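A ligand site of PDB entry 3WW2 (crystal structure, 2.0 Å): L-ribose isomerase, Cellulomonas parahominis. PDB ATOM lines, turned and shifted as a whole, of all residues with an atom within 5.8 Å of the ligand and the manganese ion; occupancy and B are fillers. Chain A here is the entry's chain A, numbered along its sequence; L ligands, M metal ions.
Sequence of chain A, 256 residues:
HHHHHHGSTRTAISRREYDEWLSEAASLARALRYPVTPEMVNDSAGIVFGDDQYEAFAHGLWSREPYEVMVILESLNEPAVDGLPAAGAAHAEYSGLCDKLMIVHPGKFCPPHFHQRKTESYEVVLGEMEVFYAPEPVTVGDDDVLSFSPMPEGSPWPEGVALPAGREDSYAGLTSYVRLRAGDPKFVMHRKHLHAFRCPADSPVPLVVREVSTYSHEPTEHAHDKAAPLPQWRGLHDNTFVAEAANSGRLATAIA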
ATOM      1  N   ILE A  47      -9.253  -8.392 -25.384  1.00  0.00           N
ATOM      2  CA  ILE A  47      -8.721  -8.945 -24.134  1.00  0.00           C
ATOM      3  C   ILE A  47      -9.297  -8.373 -22.824  1.00  0.00           C
ATOM      4  O   ILE A  47      -9.385  -7.170 -22.639  1.00  0.00           O
ATOM      5  CB  ILE A  47      -7.169  -8.769 -24.092  1.00  0.00           C
ATOM      6  CG1 ILE A  47      -6.572  -9.287 -25.398  1.00  0.00           C
ATOM      7  CG2 ILE A  47      -6.576  -9.496 -22.902  1.00  0.00           C
ATOM      8  CD1 ILE A  47      -5.065  -9.137 -25.482  1.00  0.00           C
ATOM      9  N   PHE A  49      -8.408  -8.680 -18.953  1.00  0.00           N
ATOM     10  CA  PHE A  49      -7.390  -9.184 -18.015  1.00  0.00           C
ATOM     11  C   PHE A  49      -7.893  -9.607 -16.632  1.00  0.00           C
ATOM     12  O   PHE A  49      -7.683  -8.900 -15.654  1.00  0.00           O
ATOM     13  CB  PHE A  49      -6.291  -8.127 -17.834  1.00  0.00           C
ATOM     14  CG  PHE A  49      -5.490  -7.872 -19.087  1.00  0.00           C
ATOM     15  CD1 PHE A  49      -4.476  -8.739 -19.466  1.00  0.00           C
ATOM     16  CD2 PHE A  49      -5.807  -6.792 -19.907  1.00  0.00           C
ATOM     17  CE1 PHE A  49      -3.780  -8.547 -20.661  1.00  0.00           C
ATOM     18  CE2 PHE A  49      -5.118  -6.577 -21.106  1.00  0.00           C
ATOM     19  CZ  PHE A  49      -4.097  -7.460 -21.488  1.00  0.00           C
ATOM     20  N   MET A  70      -8.721  -4.271 -23.304  1.00  0.00           N
ATOM     21  CA  MET A  70      -8.195  -3.682 -24.537  1.00  0.00           C
ATOM     22  C   MET A  70      -8.365  -4.583 -25.755  1.00  0.00           C
ATOM     23  O   MET A  70      -8.621  -5.783 -25.635  1.00  0.00           O
ATOM     24  CB  MET A  70      -6.698  -3.361 -24.359  1.00  0.00           C
ATOM     25  CG  MET A  70      -5.765  -4.561 -24.595  1.00  0.00           C
ATOM     26  SD  MET A  70      -4.033  -4.227 -24.110  1.00  0.00           S
ATOM     27  CE  MET A  70      -3.467  -3.159 -25.396  1.00  0.00           C
ATOM     28  N   ILE A  72      -6.524  -5.803 -29.421  1.00  0.00           N
ATOM     29  CA  ILE A  72      -5.269  -5.835 -30.118  1.00  0.00           C
ATOM     30  C   ILE A  72      -5.492  -6.454 -31.488  1.00  0.00           C
ATOM     31  O   ILE A  72      -6.117  -7.500 -31.611  1.00  0.00           O
ATOM     32  CB  ILE A  72      -4.216  -6.638 -29.328  1.00  0.00           C
ATOM     33  CG1 ILE A  72      -3.974  -5.957 -27.977  1.00  0.00           C
ATOM     34  CG2 ILE A  72      -2.923  -6.723 -30.115  1.00  0.00           C
ATOM     35  CD1 ILE A  72      -3.014  -6.708 -27.054  1.00  0.00           C
ATOM     36  N   LYS A 100       1.479  -4.610 -34.203  1.00  0.00           N
ATOM     37  CA  LYS A 100       0.088  -4.691 -33.785  1.00  0.00           C
ATOM     38  C   LYS A 100      -0.456  -3.331 -33.415  1.00  0.00           C
ATOM     39  O   LYS A 100       0.283  -2.438 -32.971  1.00  0.00           O
ATOM     40  CB  LYS A 100      -0.054  -5.662 -32.604  1.00  0.00           C
ATOM     41  CG  LYS A 100       0.968  -5.448 -31.504  1.00  0.00           C
ATOM     42  CD  LYS A 100       0.768  -6.428 -30.353  1.00  0.00           C
ATOM     43  CE  LYS A 100       0.785  -7.888 -30.811  1.00  0.00           C
ATOM     44  NZ  LYS A 100       0.865  -8.823 -29.636  1.00  0.00           N
ATOM     45  N   MET A 102      -3.111  -1.319 -31.046  1.00  0.00           N
ATOM     46  CA  MET A 102      -3.841  -1.472 -29.792  1.00  0.00           C
ATOM     47  C   MET A 102      -4.853  -0.365 -29.548  1.00  0.00           C
ATOM     48  O   MET A 102      -4.564   0.814 -29.768  1.00  0.00           O
ATOM     49  CB  MET A 102      -2.845  -1.553 -28.638  1.00  0.00           C
ATOM     50  CG  MET A 102      -1.831  -2.678 -28.842  1.00  0.00           C
ATOM     51  SD  MET A 102      -0.673  -2.833 -27.488  1.00  0.00           S
ATOM     52  CE  MET A 102       0.513  -1.543 -27.890  1.00  0.00           C
ATOM     53  N   CYS A 110      -3.785  -1.336 -19.851  1.00  0.00           N
ATOM     54  CA  CYS A 110      -3.092  -2.515 -20.338  1.00  0.00           C
ATOM     55  C   CYS A 110      -2.255  -2.675 -19.056  1.00  0.00           C
ATOM     56  O   CYS A 110      -1.296  -1.938 -18.857  1.00  0.00           O
ATOM     57  CB  CYS A 110      -2.176  -2.201 -21.516  1.00  0.00           C
ATOM     58  SG  CYS A 110      -0.989  -3.542 -21.806  1.00  0.00           S
ATOM     59  N   HIS A 113       3.073  -5.579 -16.355  1.00  0.00           N
ATOM     60  CA  HIS A 113       3.713  -6.832 -16.764  1.00  0.00           C
ATOM     61  C   HIS A 113       5.086  -6.541 -17.353  1.00  0.00           C
ATOM     62  O   HIS A 113       5.511  -5.382 -17.464  1.00  0.00           O
ATOM     63  CB  HIS A 113       2.871  -7.554 -17.815  1.00  0.00           C
ATOM     64  CG  HIS A 113       2.811  -6.844 -19.129  1.00  0.00           C
ATOM     65  ND1 HIS A 113       1.927  -5.808 -19.375  1.00  0.00           N
ATOM     66  CD2 HIS A 113       3.576  -6.954 -20.241  1.00  0.00           C
ATOM     67  CE1 HIS A 113       2.164  -5.309 -20.578  1.00  0.00           C
ATOM     68  NE2 HIS A 113       3.167  -5.988 -21.124  1.00  0.00           N
ATOM     69  N   HIS A 115       8.197  -8.620 -20.156  1.00  0.00           N
ATOM     70  CA  HIS A 115       8.449  -9.711 -21.077  1.00  0.00           C
ATOM     71  C   HIS A 115       9.882 -10.160 -20.849  1.00  0.00           C
ATOM     72  O   HIS A 115      10.744  -9.341 -20.515  1.00  0.00           O
ATOM     73  CB  HIS A 115       8.273  -9.236 -22.520  1.00  0.00           C
ATOM     74  CG  HIS A 115       6.936  -8.629 -22.788  1.00  0.00           C
ATOM     75  ND1 HIS A 115       5.757  -9.343 -22.696  1.00  0.00           N
ATOM     76  CD2 HIS A 115       6.574  -7.365 -23.119  1.00  0.00           C
ATOM     77  CE1 HIS A 115       4.737  -8.540 -22.946  1.00  0.00           C
ATOM     78  NE2 HIS A 115       5.209  -7.329 -23.209  1.00  0.00           N
ATOM     79  N   LYS A 118      10.521 -10.198 -25.335  1.00  0.00           N
ATOM     80  CA  LYS A 118      10.047  -9.080 -26.152  1.00  0.00           C
ATOM     81  C   LYS A 118      10.436  -7.653 -25.752  1.00  0.00           C
ATOM     82  O   LYS A 118      10.246  -7.224 -24.631  1.00  0.00           O
ATOM     83  CB  LYS A 118       8.528  -9.161 -26.297  1.00  0.00           C
ATOM     84  CG  LYS A 118       7.954  -8.258 -27.372  1.00  0.00           C
ATOM     85  CD  LYS A 118       6.440  -8.401 -27.480  1.00  0.00           C
ATOM     86  CE  LYS A 118       5.740  -7.782 -26.293  1.00  0.00           C
ATOM     87  NZ  LYS A 118       4.255  -7.783 -26.449  1.00  0.00           N
ATOM     88  N   GLU A 120       9.742  -3.783 -26.984  1.00  0.00           N
ATOM     89  CA  GLU A 120       8.740  -3.083 -27.783  1.00  0.00           C
ATOM     90  C   GLU A 120       8.927  -1.571 -27.928  1.00  0.00           C
ATOM     91  O   GLU A 120       9.728  -0.946 -27.225  1.00  0.00           O
ATOM     92  CB  GLU A 120       7.342  -3.381 -27.220  1.00  0.00           C
ATOM     93  CG  GLU A 120       7.292  -3.527 -25.700  1.00  0.00           C
ATOM     94  CD  GLU A 120       5.893  -3.895 -25.187  1.00  0.00           C
ATOM     95  OE1 GLU A 120       5.023  -3.000 -25.104  1.00  0.00           O
ATOM     96  OE2 GLU A 120       5.669  -5.079 -24.876  1.00  0.00           O
ATOM     97  N   TYR A 122       6.536   2.148 -29.044  1.00  0.00           N
ATOM     98  CA  TYR A 122       5.199   2.702 -29.174  1.00  0.00           C
ATOM     99  C   TYR A 122       5.097   3.905 -30.084  1.00  0.00           C
ATOM    100  O   TYR A 122       5.961   4.790 -30.088  1.00  0.00           O
ATOM    101  CB  TYR A 122       4.641   3.107 -27.812  1.00  0.00           C
ATOM    102  CG  TYR A 122       4.784   2.051 -26.743  1.00  0.00           C
ATOM    103  CD1 TYR A 122       4.277   0.763 -26.941  1.00  0.00           C
ATOM    104  CD2 TYR A 122       5.396   2.345 -25.529  1.00  0.00           C
ATOM    105  CE1 TYR A 122       4.394  -0.202 -25.953  1.00  0.00           C
ATOM    106  CE2 TYR A 122       5.508   1.394 -24.525  1.00  0.00           C
ATOM    107  CZ  TYR A 122       5.002   0.121 -24.736  1.00  0.00           C
ATOM    108  OH  TYR A 122       5.114  -0.823 -23.738  1.00  0.00           O
ATOM    109  N   HIS A 195       5.946  -2.572 -17.030  1.00  0.00           N
ATOM    110  CA  HIS A 195       5.262  -1.454 -17.675  1.00  0.00           C
ATOM    111  C   HIS A 195       3.748  -1.662 -17.769  1.00  0.00           C
ATOM    112  O   HIS A 195       3.234  -2.770 -17.633  1.00  0.00           O
ATOM    113  CB  HIS A 195       5.828  -1.187 -19.067  1.00  0.00           C
ATOM    114  CG  HIS A 195       5.633  -2.324 -20.025  1.00  0.00           C
ATOM    115  ND1 HIS A 195       6.412  -3.453 -20.018  1.00  0.00           N
ATOM    116  CD2 HIS A 195       4.727  -2.496 -21.022  1.00  0.00           C
ATOM    117  CE1 HIS A 195       5.999  -4.281 -20.966  1.00  0.00           C
ATOM    118  NE2 HIS A 195       4.978  -3.719 -21.590  1.00  0.00           N
ATOM    119  N   PHE A 197       0.018   0.892 -19.223  1.00  0.00           N
ATOM    120  CA  PHE A 197      -0.376   2.171 -19.784  1.00  0.00           C
ATOM    121  C   PHE A 197      -1.886   2.316 -19.880  1.00  0.00           C
ATOM    122  O   PHE A 197      -2.618   1.335 -19.903  1.00  0.00           O
ATOM    123  CB  PHE A 197       0.294   2.365 -21.147  1.00  0.00           C
ATOM    124  CG  PHE A 197      -0.198   1.431 -22.209  1.00  0.00           C
ATOM    125  CD1 PHE A 197      -1.339   1.729 -22.964  1.00  0.00           C
ATOM    126  CD2 PHE A 197       0.506   0.266 -22.511  1.00  0.00           C
ATOM    127  CE1 PHE A 197      -1.777   0.882 -23.983  1.00  0.00           C
ATOM    128  CE2 PHE A 197       0.077  -0.583 -23.531  1.00  0.00           C
ATOM    129  CZ  PHE A 197      -1.059  -0.272 -24.271  1.00  0.00           C
ATOM    130  N   GLU A 211       2.145  -0.837 -31.966  1.00  0.00           N
ATOM    131  CA  GLU A 211       3.266  -1.459 -31.283  1.00  0.00           C
ATOM    132  C   GLU A 211       4.147  -2.183 -32.304  1.00  0.00           C
ATOM    133  O   GLU A 211       3.668  -2.994 -33.098  1.00  0.00           O
ATOM    134  CB  GLU A 211       2.785  -2.477 -30.240  1.00  0.00           C
ATOM    135  CG  GLU A 211       3.922  -3.240 -29.551  1.00  0.00           C
ATOM    136  CD  GLU A 211       3.435  -4.303 -28.562  1.00  0.00           C
ATOM    137  OE1 GLU A 211       2.736  -3.945 -27.586  1.00  0.00           O
ATOM    138  OE2 GLU A 211       3.747  -5.491 -28.776  1.00  0.00           O
ATOM    139  N   SER A 216       6.229 -11.999 -30.716  1.00  0.00           N
ATOM    140  CA  SER A 216       5.282 -12.077 -29.619  1.00  0.00           C
ATOM    141  C   SER A 216       4.854 -13.523 -29.320  1.00  0.00           C
ATOM    142  O   SER A 216       4.040 -14.101 -30.032  1.00  0.00           O
ATOM    143  CB  SER A 216       4.060 -11.219 -29.972  1.00  0.00           C
ATOM    144  OG  SER A 216       3.108 -11.227 -28.933  1.00  0.00           O
ATOM    145  N   GLU A 218       2.674 -15.721 -27.593  1.00  0.00           N
ATOM    146  CA  GLU A 218       1.398 -15.715 -26.867  1.00  0.00           C
ATOM    147  C   GLU A 218       0.534 -16.894 -27.314  1.00  0.00           C
ATOM    148  O   GLU A 218      -0.255 -16.775 -28.242  1.00  0.00           O
ATOM    149  CB  GLU A 218       0.643 -14.406 -27.140  1.00  0.00           C
ATOM    150  CG  GLU A 218       1.399 -13.160 -26.743  1.00  0.00           C
ATOM    151  CD  GLU A 218       0.673 -11.886 -27.116  1.00  0.00           C
ATOM    152  OE1 GLU A 218       0.378 -11.693 -28.326  1.00  0.00           O
ATOM    153  OE2 GLU A 218       0.389 -11.069 -26.210  1.00  0.00           O
ATOM    154  N   ASN A 239       4.710 -13.355 -21.449  1.00  0.00           N
ATOM    155  CA  ASN A 239       4.058 -12.275 -20.704  1.00  0.00           C
ATOM    156  C   ASN A 239       3.876 -12.644 -19.238  1.00  0.00           C
ATOM    157  O   ASN A 239       3.208 -13.618 -18.925  1.00  0.00           O
ATOM    158  CB  ASN A 239       2.684 -11.935 -21.287  1.00  0.00           C
ATOM    159  CG  ASN A 239       2.712 -11.657 -22.777  1.00  0.00           C
ATOM    160  OD1 ASN A 239       3.697 -11.128 -23.297  1.00  0.00           O
ATOM    161  ND2 ASN A 239       1.626 -12.002 -23.465  1.00  0.00           N
ATOM    162  N   PHE A 241       2.373 -11.128 -15.805  1.00  0.00           N
ATOM    163  CA  PHE A 241       1.617 -10.054 -15.197  1.00  0.00           C
ATOM    164  C   PHE A 241       1.847 -10.001 -13.703  1.00  0.00           C
ATOM    165  O   PHE A 241       2.022 -11.034 -13.052  1.00  0.00           O
ATOM    166  CB  PHE A 241       0.121 -10.223 -15.490  1.00  0.00           C
ATOM    167  CG  PHE A 241      -0.236 -10.110 -16.936  1.00  0.00           C
ATOM    168  CD1 PHE A 241      -0.253 -11.234 -17.758  1.00  0.00           C
ATOM    169  CD2 PHE A 241      -0.492  -8.857 -17.504  1.00  0.00           C
ATOM    170  CE1 PHE A 241      -0.524 -11.122 -19.123  1.00  0.00           C
ATOM    171  CE2 PHE A 241      -0.763  -8.738 -18.875  1.00  0.00           C
ATOM    172  CZ  PHE A 241      -0.778  -9.871 -19.677  1.00  0.00           C
ATOM    173  N   ARG A 250      -5.846 -13.418 -19.572  1.00  0.00           N
ATOM    174  CA  ARG A 250      -5.278 -12.964 -20.839  1.00  0.00           C
ATOM    175  C   ARG A 250      -5.246 -14.051 -21.923  1.00  0.00           C
ATOM    176  O   ARG A 250      -5.031 -13.744 -23.106  1.00  0.00           O
ATOM    177  CB  ARG A 250      -3.853 -12.424 -20.594  1.00  0.00           C
ATOM    178  CG  ARG A 250      -3.297 -11.511 -21.693  1.00  0.00           C
ATOM    179  CD  ARG A 250      -2.772 -12.273 -22.906  1.00  0.00           C
ATOM    180  NE  ARG A 250      -2.647 -11.408 -24.073  1.00  0.00           N
ATOM    181  CZ  ARG A 250      -2.337 -11.832 -25.289  1.00  0.00           C
ATOM    182  NH1 ARG A 250      -2.252 -10.977 -26.300  1.00  0.00           N
ATOM    183  NH2 ARG A 250      -2.118 -13.124 -25.507  1.00  0.00           N
HETATM  184  C1  LIG L   1       1.370  -4.365 -24.329  1.00  0.00           C
HETATM  185  O1  LIG L   1       2.573  -3.752 -23.875  1.00  0.00           O
HETATM  186  C2  LIG L   1       1.597  -5.813 -24.714  1.00  0.00           C
HETATM  187  O2  LIG L   1       2.980  -6.024 -24.966  1.00  0.00           O
HETATM  188  C3  LIG L   1       0.761  -6.281 -25.900  1.00  0.00           C
HETATM  189  O3  LIG L   1       1.560  -6.320 -27.081  1.00  0.00           O
HETATM  190  C4  LIG L   1       0.328  -7.703 -25.526  1.00  0.00           C
HETATM  191  O4  LIG L   1       1.164  -8.645 -26.176  1.00  0.00           O
HETATM  192  C5  LIG L   1       0.532  -7.804 -24.016  1.00  0.00           C
HETATM  193  O5  LIG L   1       1.229  -6.621 -23.588  1.00  0.00           O
HETATM  194  C6  LIG L   1      -0.772  -7.876 -23.243  1.00  0.00           C
HETATM  195  O6  LIG L   1      -1.087  -9.223 -22.928  1.00  0.00           O
HETATM  196 MN    MN M   1       4.196  -5.388 -23.114  1.00  0.00          MN
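The side-chain carboxylate of Glu 218 lies within hydrogen-bond range of an oxygen (O4) of the ligand. NZ of Lys 118 lies within hydrogen-bond range of O3 of the ligand (3.1 Å). OE1 of Glu 211 is in hydrogen-bond range of O3 of the ligand, at 2.7 Å. NE of Arg 250 is in hydrogen-bond range of O6 of the ligand (2.9 Å). The side-chain amino group (NZ) of Lys 100 lies within hydrogen-bond range of an oxygen (O4) of the ligand (3.5 Å).
NE2 of His 115 sits close to NZ of Lys 118 (3.4 Å). ND1 of His 115 is in hydrogen-bond range of OD1 of Asn 239 (2.8 Å). OE2 of Glu 120 sits close to NZ of Lys 118 (3.4 Å). OE1 of Glu 218 lies within salt-bridge range of NZ of Lys 100 (3.2 Å). OE2 of Glu 218 sits at hydrogen-bond distance from ND2 of Asn 239 (3.2 Å). OE2 of Glu 211 lies within salt-bridge range of NZ of Lys 118, 3.3 Å away. The backbone NH of Glu 211 sits at hydrogen-bond distance from the backbone carbonyl oxygen of Lys 100, 2.7 Å away. The backbone NH (N) of Cys 110 sits at hydrogen-bond distance from the backbone carbonyl oxygen (O) of Phe 197, at 2.9 Å.
Phe 49 touches the ligand (CE1 to O6, 3.6 Å). CD1 of Ile 72 touches C4 of the ligand, at 3.8 Å. Cys 110 touches the ligand. Tyr 122 touches the ligand. Asn 239 touches the ligand. Phe 241 touches the ligand. Hydrophobic or aromatic side chains within 4 Å of the ligand: Phe 49, Ile 72, His 113, His 115, His 195 and Phe 241. Within 4 Å of the ligand: Phe 49, Ile 72, Lys 100, Cys 110, His 113, His 115, Lys 118, Glu 120, Tyr 122, His 195, Glu 211, Glu 218, Asn 239, Phe 241 and Arg 250. Along chain A the residues within 4 Å of the ligand span positions 49 to 250.
Of the 20 residues printed, 4 come within 4 Å of the manganese ion. The nearest printed residue that does not touch the manganese ion is Lys 118 (4.1 Å).
The manganese ion is bound by a ring nitrogen (NE2) of His 115 (2.2 Å), an oxygen (O2) of the ligand (2.3 Å), the side-chain carboxylate (OE2) of Glu 120 (2.3 Å), a ring nitrogen (NE2) of His 113 (2.3 Å), a ring nitrogen (NE2) of His 195 (2.4 Å) and an oxygen (O1) of the ligand (2.4 Å).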
